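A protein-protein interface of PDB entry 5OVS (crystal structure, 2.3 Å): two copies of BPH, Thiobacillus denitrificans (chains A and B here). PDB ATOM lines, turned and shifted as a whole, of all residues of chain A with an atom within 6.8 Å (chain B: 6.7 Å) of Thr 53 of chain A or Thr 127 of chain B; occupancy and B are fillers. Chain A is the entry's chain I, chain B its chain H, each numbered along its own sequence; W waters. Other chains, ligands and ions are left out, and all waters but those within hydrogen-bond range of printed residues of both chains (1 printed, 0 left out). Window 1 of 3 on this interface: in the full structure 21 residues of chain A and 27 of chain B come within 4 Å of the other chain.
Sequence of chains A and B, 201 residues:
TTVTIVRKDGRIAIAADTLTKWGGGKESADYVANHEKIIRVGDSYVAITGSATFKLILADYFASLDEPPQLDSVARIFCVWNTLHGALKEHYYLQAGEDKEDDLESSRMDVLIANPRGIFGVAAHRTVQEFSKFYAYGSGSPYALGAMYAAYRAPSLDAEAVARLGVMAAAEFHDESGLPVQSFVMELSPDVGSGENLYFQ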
ATOM      1  N   THR A  20      -8.975  -7.227 -18.159  1.00  0.00           N
ATOM      2  CA  THR A  20      -9.730  -8.387 -18.608  1.00  0.00           C
ATOM      3  C   THR A  20      -9.399  -9.619 -17.766  1.00  0.00           C
ATOM      4  O   THR A  20      -8.260  -9.829 -17.338  1.00  0.00           O
ATOM      5  CB  THR A  20      -9.487  -8.658 -20.100  1.00  0.00           C
ATOM      6  OG1 THR A  20      -9.983  -7.544 -20.842  1.00  0.00           O
ATOM      7  CG2 THR A  20     -10.219  -9.897 -20.570  1.00  0.00           C
ATOM      8  N   GLU A  27      -5.640 -10.135 -17.029  1.00  0.00           N
ATOM      9  CA  GLU A  27      -5.033  -9.706 -18.268  1.00  0.00           C
ATOM     10  C   GLU A  27      -5.088  -8.170 -18.275  1.00  0.00           C
ATOM     11  O   GLU A  27      -6.032  -7.562 -18.778  1.00  0.00           O
ATOM     12  CB  GLU A  27      -5.790 -10.330 -19.439  1.00  0.00           C
ATOM     13  CG  GLU A  27      -5.797 -11.853 -19.365  1.00  0.00           C
ATOM     14  CD  GLU A  27      -6.675 -12.547 -20.404  1.00  0.00           C
ATOM     15  OE1 GLU A  27      -7.646 -11.939 -20.892  1.00  0.00           O
ATOM     16  OE2 GLU A  27      -6.407 -13.731 -20.716  1.00  0.00           O
ATOM     17  N   ASN A  34      -5.062  -4.054 -26.732  1.00  0.00           N
ATOM     18  CA  ASN A  34      -6.400  -3.570 -27.047  1.00  0.00           C
ATOM     19  C   ASN A  34      -7.310  -3.650 -25.828  1.00  0.00           C
ATOM     20  O   ASN A  34      -8.340  -4.309 -25.851  1.00  0.00           O
ATOM     21  CB  ASN A  34      -6.982  -4.335 -28.249  1.00  0.00           C
ATOM     22  CG  ASN A  34      -7.073  -5.841 -28.018  1.00  0.00           C
ATOM     23  OD1 ASN A  34      -6.110  -6.481 -27.590  1.00  0.00           O
ATOM     24  ND2 ASN A  34      -8.236  -6.414 -28.316  1.00  0.00           N
ATOM     25  N   ILE A  48     -18.499  -0.661 -22.540  1.00  0.00           N
ATOM     26  CA  ILE A  48     -19.085  -1.999 -22.633  1.00  0.00           C
ATOM     27  C   ILE A  48     -18.667  -2.925 -21.474  1.00  0.00           C
ATOM     28  O   ILE A  48     -17.509  -2.957 -21.085  1.00  0.00           O
ATOM     29  CB  ILE A  48     -18.731  -2.624 -23.999  1.00  0.00           C
ATOM     30  CG1 ILE A  48     -19.287  -1.734 -25.136  1.00  0.00           C
ATOM     31  CG2 ILE A  48     -19.299  -4.033 -24.121  1.00  0.00           C
ATOM     32  CD1 ILE A  48     -18.655  -1.963 -26.493  1.00  0.00           C
ATOM     33  N   GLY A  50     -19.389  -7.053 -19.654  1.00  0.00           N
ATOM     34  CA  GLY A  50     -19.644  -8.430 -20.052  1.00  0.00           C
ATOM     35  C   GLY A  50     -18.432  -8.960 -20.770  1.00  0.00           C
ATOM     36  O   GLY A  50     -17.376  -8.351 -20.716  1.00  0.00           O
ATOM     37  N   SER A  51     -18.572 -10.094 -21.446  1.00  0.00           N
ATOM     38  CA  SER A  51     -17.439 -10.715 -22.156  1.00  0.00           C
ATOM     39  C   SER A  51     -16.614  -9.713 -22.951  1.00  0.00           C
ATOM     40  O   SER A  51     -17.158  -8.844 -23.631  1.00  0.00           O
ATOM     41  CB  SER A  51     -17.933 -11.797 -23.117  1.00  0.00           C
ATOM     42  OG  SER A  51     -16.973 -12.049 -24.133  1.00  0.00           O
ATOM     43  N   ALA A  52     -15.298  -9.865 -22.897  1.00  0.00           N
ATOM     44  CA  ALA A  52     -14.400  -8.969 -23.627  1.00  0.00           C
ATOM     45  C   ALA A  52     -14.570  -9.062 -25.160  1.00  0.00           C
ATOM     46  O   ALA A  52     -14.007  -8.238 -25.888  1.00  0.00           O
ATOM     47  CB  ALA A  52     -12.962  -9.242 -23.234  1.00  0.00           C
ATOM     48  N   THR A  53     -15.336 -10.056 -25.629  1.00  0.00           N
ATOM     49  CA  THR A  53     -15.662 -10.213 -27.046  1.00  0.00           C
ATOM     50  C   THR A  53     -16.690  -9.184 -27.548  1.00  0.00           C
ATOM     51  O   THR A  53     -16.760  -8.898 -28.751  1.00  0.00           O
ATOM     52  CB  THR A  53     -16.213 -11.625 -27.331  1.00  0.00           C
ATOM     53  OG1 THR A  53     -15.258 -12.614 -26.926  1.00  0.00           O
ATOM     54  CG2 THR A  53     -16.512 -11.816 -28.811  1.00  0.00           C
ATOM     55  N   PHE A  54     -17.482  -8.624 -26.636  1.00  0.00           N
ATOM     56  CA  PHE A  54     -18.561  -7.721 -27.031  1.00  0.00           C
ATOM     57  C   PHE A  54     -18.073  -6.437 -27.697  1.00  0.00           C
ATOM     58  O   PHE A  54     -18.678  -5.960 -28.659  1.00  0.00           O
ATOM     59  CB  PHE A  54     -19.471  -7.395 -25.839  1.00  0.00           C
ATOM     60  CG  PHE A  54     -20.460  -8.477 -25.532  1.00  0.00           C
ATOM     61  CD1 PHE A  54     -21.479  -8.767 -26.432  1.00  0.00           C
ATOM     62  CD2 PHE A  54     -20.376  -9.214 -24.350  1.00  0.00           C
ATOM     63  CE1 PHE A  54     -22.402  -9.767 -26.159  1.00  0.00           C
ATOM     64  CE2 PHE A  54     -21.296 -10.213 -24.075  1.00  0.00           C
ATOM     65  CZ  PHE A  54     -22.306 -10.490 -24.979  1.00  0.00           C
ATOM     66  N   LYS A  55     -16.984  -5.872 -27.198  1.00  0.00           N
ATOM     67  CA  LYS A  55     -16.447  -4.665 -27.814  1.00  0.00           C
ATOM     68  C   LYS A  55     -16.074  -4.873 -29.286  1.00  0.00           C
ATOM     69  O   LYS A  55     -16.180  -3.947 -30.082  1.00  0.00           O
ATOM     70  CB  LYS A  55     -15.253  -4.139 -27.025  1.00  0.00           C
ATOM     71  CG  LYS A  55     -13.992  -4.975 -27.128  1.00  0.00           C
ATOM     72  CD  LYS A  55     -12.922  -4.360 -26.245  1.00  0.00           C
ATOM     73  CE  LYS A  55     -11.840  -5.352 -25.867  1.00  0.00           C
ATOM     74  NZ  LYS A  55     -11.606  -5.326 -24.395  1.00  0.00           N
ATOM     75  N   LEU A  56     -15.654  -6.090 -29.628  1.00  0.00           N
ATOM     76  CA  LEU A  56     -15.267  -6.436 -30.999  1.00  0.00           C
ATOM     77  C   LEU A  56     -16.504  -6.641 -31.856  1.00  0.00           C
ATOM     78  O   LEU A  56     -16.556  -6.192 -33.007  1.00  0.00           O
ATOM     79  CB  LEU A  56     -14.441  -7.716 -31.012  1.00  0.00           C
ATOM     80  CG  LEU A  56     -13.229  -7.732 -30.079  1.00  0.00           C
ATOM     81  CD1 LEU A  56     -12.764  -9.150 -29.800  1.00  0.00           C
ATOM     82  CD2 LEU A  56     -12.106  -6.886 -30.664  1.00  0.00           C
ATOM     83  N   ILE A  57     -17.491  -7.331 -31.280  1.00  0.00           N
ATOM     84  CA  ILE A  57     -18.765  -7.584 -31.934  1.00  0.00           C
ATOM     85  C   ILE A  57     -19.436  -6.260 -32.318  1.00  0.00           C
ATOM     86  O   ILE A  57     -19.785  -6.060 -33.491  1.00  0.00           O
ATOM     87  CB  ILE A  57     -19.690  -8.448 -31.034  1.00  0.00           C
ATOM     88  CG1 ILE A  57     -19.203  -9.895 -31.012  1.00  0.00           C
ATOM     89  CG2 ILE A  57     -21.144  -8.389 -31.511  1.00  0.00           C
ATOM     90  CD1 ILE A  57     -19.908 -10.758 -29.989  1.00  0.00           C
ATOM     91  N   LEU A  58     -19.594  -5.353 -31.348  1.00  0.00           N
ATOM     92  CA  LEU A  58     -20.259  -4.075 -31.604  1.00  0.00           C
ATOM     93  C   LEU A  58     -19.495  -3.222 -32.587  1.00  0.00           C
ATOM     94  O   LEU A  58     -20.089  -2.641 -33.492  1.00  0.00           O
ATOM     95  CB  LEU A  58     -20.482  -3.261 -30.332  1.00  0.00           C
ATOM     96  CG  LEU A  58     -21.376  -3.822 -29.218  1.00  0.00           C
ATOM     97  CD1 LEU A  58     -22.194  -2.694 -28.608  1.00  0.00           C
ATOM     98  CD2 LEU A  58     -22.302  -4.929 -29.674  1.00  0.00           C
ATOM     99  N   TYR A  92     -23.438 -13.574 -34.355  1.00  0.00           N
ATOM    100  CA  TYR A  92     -22.351 -13.537 -33.372  1.00  0.00           C
ATOM    101  C   TYR A  92     -22.440 -14.604 -32.295  1.00  0.00           C
ATOM    102  O   TYR A  92     -21.654 -14.595 -31.355  1.00  0.00           O
ATOM    103  CB  TYR A  92     -22.260 -12.137 -32.742  1.00  0.00           C
ATOM    104  CG  TYR A  92     -21.894 -11.082 -33.754  1.00  0.00           C
ATOM    105  CD1 TYR A  92     -20.652 -11.100 -34.377  1.00  0.00           C
ATOM    106  CD2 TYR A  92     -22.801 -10.098 -34.126  1.00  0.00           C
ATOM    107  CE1 TYR A  92     -20.311 -10.155 -35.324  1.00  0.00           C
ATOM    108  CE2 TYR A  92     -22.467  -9.147 -35.073  1.00  0.00           C
ATOM    109  CZ  TYR A  92     -21.221  -9.185 -35.666  1.00  0.00           C
ATOM    110  OH  TYR A  92     -20.884  -8.257 -36.606  1.00  0.00           O
ATOM    111  N   PHE B  78     -10.749 -11.284 -35.533  1.00  0.00           N
ATOM    112  CA  PHE B  78     -12.102 -11.493 -35.050  1.00  0.00           C
ATOM    113  C   PHE B  78     -13.045 -11.874 -36.186  1.00  0.00           C
ATOM    114  O   PHE B  78     -13.848 -12.798 -36.059  1.00  0.00           O
ATOM    115  CB  PHE B  78     -12.660 -10.259 -34.347  1.00  0.00           C
ATOM    116  CG  PHE B  78     -14.102 -10.408 -33.994  1.00  0.00           C
ATOM    117  CD1 PHE B  78     -14.479 -11.255 -32.962  1.00  0.00           C
ATOM    118  CD2 PHE B  78     -15.086  -9.784 -34.748  1.00  0.00           C
ATOM    119  CE1 PHE B  78     -15.811 -11.441 -32.651  1.00  0.00           C
ATOM    120  CE2 PHE B  78     -16.425  -9.965 -34.445  1.00  0.00           C
ATOM    121  CZ  PHE B  78     -16.787 -10.799 -33.393  1.00  0.00           C
ATOM    122  N   ASN B  82     -14.897 -15.468 -36.122  1.00  0.00           N
ATOM    123  CA  ASN B  82     -16.349 -15.482 -36.047  1.00  0.00           C
ATOM    124  C   ASN B  82     -16.911 -16.381 -37.142  1.00  0.00           C
ATOM    125  O   ASN B  82     -17.744 -17.244 -36.870  1.00  0.00           O
ATOM    126  CB  ASN B  82     -16.933 -14.071 -36.148  1.00  0.00           C
ATOM    127  CG  ASN B  82     -18.380 -14.016 -35.705  1.00  0.00           C
ATOM    128  OD1 ASN B  82     -18.698 -14.364 -34.569  1.00  0.00           O
ATOM    129  ND2 ASN B  82     -19.266 -13.586 -36.598  1.00  0.00           N
ATOM    130  N   LEU B 104     -21.535 -16.158 -24.870  1.00  0.00           N
ATOM    131  CA  LEU B 104     -21.445 -16.524 -26.274  1.00  0.00           C
ATOM    132  C   LEU B 104     -21.154 -18.016 -26.390  1.00  0.00           C
ATOM    133  O   LEU B 104     -20.644 -18.650 -25.443  1.00  0.00           O
ATOM    134  CB  LEU B 104     -20.315 -15.726 -26.925  1.00  0.00           C
ATOM    135  CG  LEU B 104     -20.408 -14.213 -26.717  1.00  0.00           C
ATOM    136  CD1 LEU B 104     -19.066 -13.549 -26.981  1.00  0.00           C
ATOM    137  CD2 LEU B 104     -21.489 -13.613 -27.605  1.00  0.00           C
ATOM    138  N   GLY B 121      -3.970 -13.311 -29.706  1.00  0.00           N
ATOM    139  CA  GLY B 121      -4.633 -14.499 -29.173  1.00  0.00           C
ATOM    140  C   GLY B 121      -6.135 -14.456 -29.362  1.00  0.00           C
ATOM    141  O   GLY B 121      -6.753 -13.388 -29.283  1.00  0.00           O
ATOM    142  N   VAL B 122      -6.713 -15.628 -29.616  1.00  0.00           N
ATOM    143  CA  VAL B 122      -8.158 -15.796 -29.624  1.00  0.00           C
ATOM    144  C   VAL B 122      -8.538 -16.871 -28.595  1.00  0.00           C
ATOM    145  O   VAL B 122      -8.059 -18.006 -28.653  1.00  0.00           O
ATOM    146  CB  VAL B 122      -8.680 -16.171 -31.024  1.00  0.00           C
ATOM    147  CG1 VAL B 122     -10.195 -16.055 -31.071  1.00  0.00           C
ATOM    148  CG2 VAL B 122      -8.052 -15.271 -32.086  1.00  0.00           C
ATOM    149  N   ALA B 123      -9.355 -16.489 -27.620  1.00  0.00           N
ATOM    150  CA  ALA B 123      -9.863 -17.442 -26.632  1.00  0.00           C
ATOM    151  C   ALA B 123     -11.137 -18.073 -27.161  1.00  0.00           C
ATOM    152  O   ALA B 123     -11.768 -17.538 -28.060  1.00  0.00           O
ATOM    153  CB  ALA B 123     -10.124 -16.764 -25.286  1.00  0.00           C
ATOM    154  N   ALA B 124     -11.509 -19.202 -26.569  1.00  0.00           N
ATOM    155  CA  ALA B 124     -12.700 -19.983 -26.958  1.00  0.00           C
ATOM    156  C   ALA B 124     -13.951 -19.163 -27.311  1.00  0.00           C
ATOM    157  O   ALA B 124     -14.729 -19.564 -28.172  1.00  0.00           O
ATOM    158  CB  ALA B 124     -13.038 -20.970 -25.857  1.00  0.00           C
ATOM    159  N   HIS B 125     -14.146 -18.029 -26.647  1.00  0.00           N
ATOM    160  CA  HIS B 125     -15.320 -17.211 -26.889  1.00  0.00           C
ATOM    161  C   HIS B 125     -15.055 -16.050 -27.867  1.00  0.00           C
ATOM    162  O   HIS B 125     -15.722 -15.023 -27.806  1.00  0.00           O
ATOM    163  CB  HIS B 125     -15.878 -16.738 -25.543  1.00  0.00           C
ATOM    164  CG  HIS B 125     -16.303 -17.868 -24.652  1.00  0.00           C
ATOM    165  ND1 HIS B 125     -15.528 -18.333 -23.608  1.00  0.00           N
ATOM    166  CD2 HIS B 125     -17.408 -18.652 -24.673  1.00  0.00           C
ATOM    167  CE1 HIS B 125     -16.147 -19.338 -23.014  1.00  0.00           C
ATOM    168  NE2 HIS B 125     -17.291 -19.550 -23.639  1.00  0.00           N
ATOM    169  N   ARG B 126     -14.089 -16.247 -28.768  1.00  0.00           N
ATOM    170  CA  ARG B 126     -13.726 -15.307 -29.843  1.00  0.00           C
ATOM    171  C   ARG B 126     -13.193 -13.966 -29.355  1.00  0.00           C
ATOM    172  O   ARG B 126     -13.237 -12.954 -30.067  1.00  0.00           O
ATOM    173  CB  ARG B 126     -14.864 -15.166 -30.868  1.00  0.00           C
ATOM    174  CG  ARG B 126     -14.951 -16.418 -31.742  1.00  0.00           C
ATOM    175  CD  ARG B 126     -16.289 -16.642 -32.431  1.00  0.00           C
ATOM    176  NE  ARG B 126     -17.440 -16.533 -31.539  1.00  0.00           N
ATOM    177  CZ  ARG B 126     -17.759 -17.391 -30.566  1.00  0.00           C
ATOM    178  NH1 ARG B 126     -17.009 -18.466 -30.304  1.00  0.00           N
ATOM    179  NH2 ARG B 126     -18.846 -17.153 -29.833  1.00  0.00           N
ATOM    180  N   THR B 127     -12.634 -14.007 -28.150  1.00  0.00           N
ATOM    181  CA  THR B 127     -11.989 -12.879 -27.524  1.00  0.00           C
ATOM    182  C   THR B 127     -10.597 -12.680 -28.132  1.00  0.00           C
ATOM    183  O   THR B 127      -9.623 -13.338 -27.724  1.00  0.00           O
ATOM    184  CB  THR B 127     -11.849 -13.130 -26.020  1.00  0.00           C
ATOM    185  OG1 THR B 127     -13.092 -13.634 -25.494  1.00  0.00           O
ATOM    186  CG2 THR B 127     -11.447 -11.849 -25.312  1.00  0.00           C
ATOM    187  N   VAL B 128     -10.518 -11.788 -29.126  1.00  0.00           N
ATOM    188  CA  VAL B 128      -9.254 -11.476 -29.788  1.00  0.00           C
ATOM    189  C   VAL B 128      -8.504 -10.415 -28.987  1.00  0.00           C
ATOM    190  O   VAL B 128      -9.039  -9.334 -28.721  1.00  0.00           O
ATOM    191  CB  VAL B 128      -9.447 -10.941 -31.219  1.00  0.00           C
ATOM    192  CG1 VAL B 128      -8.095 -10.805 -31.916  1.00  0.00           C
ATOM    193  CG2 VAL B 128     -10.394 -11.828 -32.027  1.00  0.00           C
ATOM    194  N   GLN B 129      -7.266 -10.729 -28.606  1.00  0.00           N
ATOM    195  CA  GLN B 129      -6.379  -9.753 -27.984  1.00  0.00           C
ATOM    196  C   GLN B 129      -5.059  -9.645 -28.739  1.00  0.00           C
ATOM    197  O   GLN B 129      -4.523 -10.656 -29.179  1.00  0.00           O
ATOM    198  CB  GLN B 129      -6.123 -10.158 -26.541  1.00  0.00           C
ATOM    199  CG  GLN B 129      -7.359  -9.988 -25.674  1.00  0.00           C
ATOM    200  CD  GLN B 129      -7.268 -10.772 -24.388  1.00  0.00           C
ATOM    201  OE1 GLN B 129      -6.867 -11.934 -24.380  1.00  0.00           O
ATOM    202  NE2 GLN B 129      -7.655 -10.144 -23.295  1.00  0.00           N
ATOM    203  N   TYR B 137      -1.680 -19.951 -23.456  1.00  0.00           N
ATOM    204  CA  TYR B 137      -2.999 -20.517 -23.413  1.00  0.00           C
ATOM    205  C   TYR B 137      -2.847 -22.015 -23.255  1.00  0.00           C
ATOM    206  O   TYR B 137      -1.762 -22.560 -23.486  1.00  0.00           O
ATOM    207  CB  TYR B 137      -3.740 -20.211 -24.717  1.00  0.00           C
ATOM    208  CG  TYR B 137      -4.563 -18.936 -24.734  1.00  0.00           C
ATOM    209  CD1 TYR B 137      -5.175 -18.456 -23.580  1.00  0.00           C
ATOM    210  CD2 TYR B 137      -4.780 -18.238 -25.928  1.00  0.00           C
ATOM    211  CE1 TYR B 137      -5.948 -17.312 -23.600  1.00  0.00           C
ATOM    212  CE2 TYR B 137      -5.548 -17.080 -25.949  1.00  0.00           C
ATOM    213  CZ  TYR B 137      -6.129 -16.626 -24.778  1.00  0.00           C
ATOM    214  OH  TYR B 137      -6.901 -15.487 -24.743  1.00  0.00           O
HETATM  215  O   HOH W   1     -18.997 -14.259 -31.601  1.00  0.00           O
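Water W1 lies within hydrogen-bond range of O of Tyr 92 of chain A, NE of Arg 126 of chain B and OD1 of Asn 82 of chain B.
Hydrophobic or aromatic side chains of chain A within 4 Å of the printed part of chain B: Ala 52, Leu 56, Ile 57 and Tyr 92.
Of the 13 printed residues of chain B, 8 touch a printed residue of chain A.
Hydrophobic or aromatic side chains of chain B within 4 Å of the printed part of chain A: Phe 78 and Leu 104.
Among the printed residues, no Asp or Glu carboxylate lies within 4 Å of a Lys or Arg side-chain nitrogen of the other chain.
No position is printed for both chains.
Of the 17 pairs that touch across the chains among the printed residues, none has its exchanged pair printed and touching as well.
Ile 48 of chain A touches none of the printed residues of chain B.
Of chain B, only Phe 78, Leu 104, His 125, Arg 126 and Thr 127 come within 4 Å of Thr 53 of chain A.
Printed residues of chain A within 4 Å of Asn 82 of chain B: Tyr 92.
Of the printed residues of chain A, Leu 104 of chain B touches Ser 51, Thr 53 and Tyr 92.
The nearest printed residue of chain A that does not touch Gln 129 of chain B is Ala 52 of chain A (5.4 Å).
The backbone NH (N) of Gly 121 of chain B lies within hydrogen-bond range of the backbone carbonyl oxygen (O) of Gln 129 of chain B (2.8 Å).
O of Ala 124 of chain B lies within hydrogen-bond range of NH1 of Arg 126 of chain B.
The backbone carbonyl oxygen (O) of Thr 20 of chain A lies within hydrogen-bond range of the backbone NH (N) of Glu 27 of chain A (2.7 Å).
The side-chain hydroxyl (OG) of Ser 51 of chain A is in hydrogen-bond range of the backbone NH (N) of Thr 53 of chain A (3.0 Å).
The backbone carbonyl oxygen of His 125 of chain B sits at hydrogen-bond distance from the side-chain hydroxyl of Thr 53 of chain A, at 2.6 Å.
OG1 of Thr 127 of chain B sits at hydrogen-bond distance from OG1 of Thr 53 of chain A.
The side-chain amide nitrogen (ND2) of Asn 34 of chain A is in hydrogen-bond range of the backbone carbonyl oxygen (O) of Val 128 of chain B (3.1 Å).
The side-chain carboxylate (OE1) of Glu 27 of chain A sits at hydrogen-bond distance from the side-chain amide nitrogen (NE2) of Gln 129 of chain B.
Among the printed residues, pairs that only touch across the chains: Thr 20 of chain A with Gln 129 of chain B, Asn 34 of chain A with Gln 129 of chain B, Ser 51 of chain A with Leu 104 of chain B, Ala 52 of chain A with Thr 127 of chain B, Thr 53 of chain A with Phe 78 of chain B, Thr 53 of chain A with Leu 104 of chain B, Thr 53 of chain A with Arg 126 of chain B, Leu 56 of chain A with Arg 126 of chain B, Leu 56 of chain A with Val 128 of chain B, Ile 57 of chain A with Phe 78 of chain B, Tyr 92 of chain A with Phe 78 of chain B, Tyr 92 of chain A with Asn 82 of chain B and Tyr 92 of chain A with Leu 104 of chain B.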
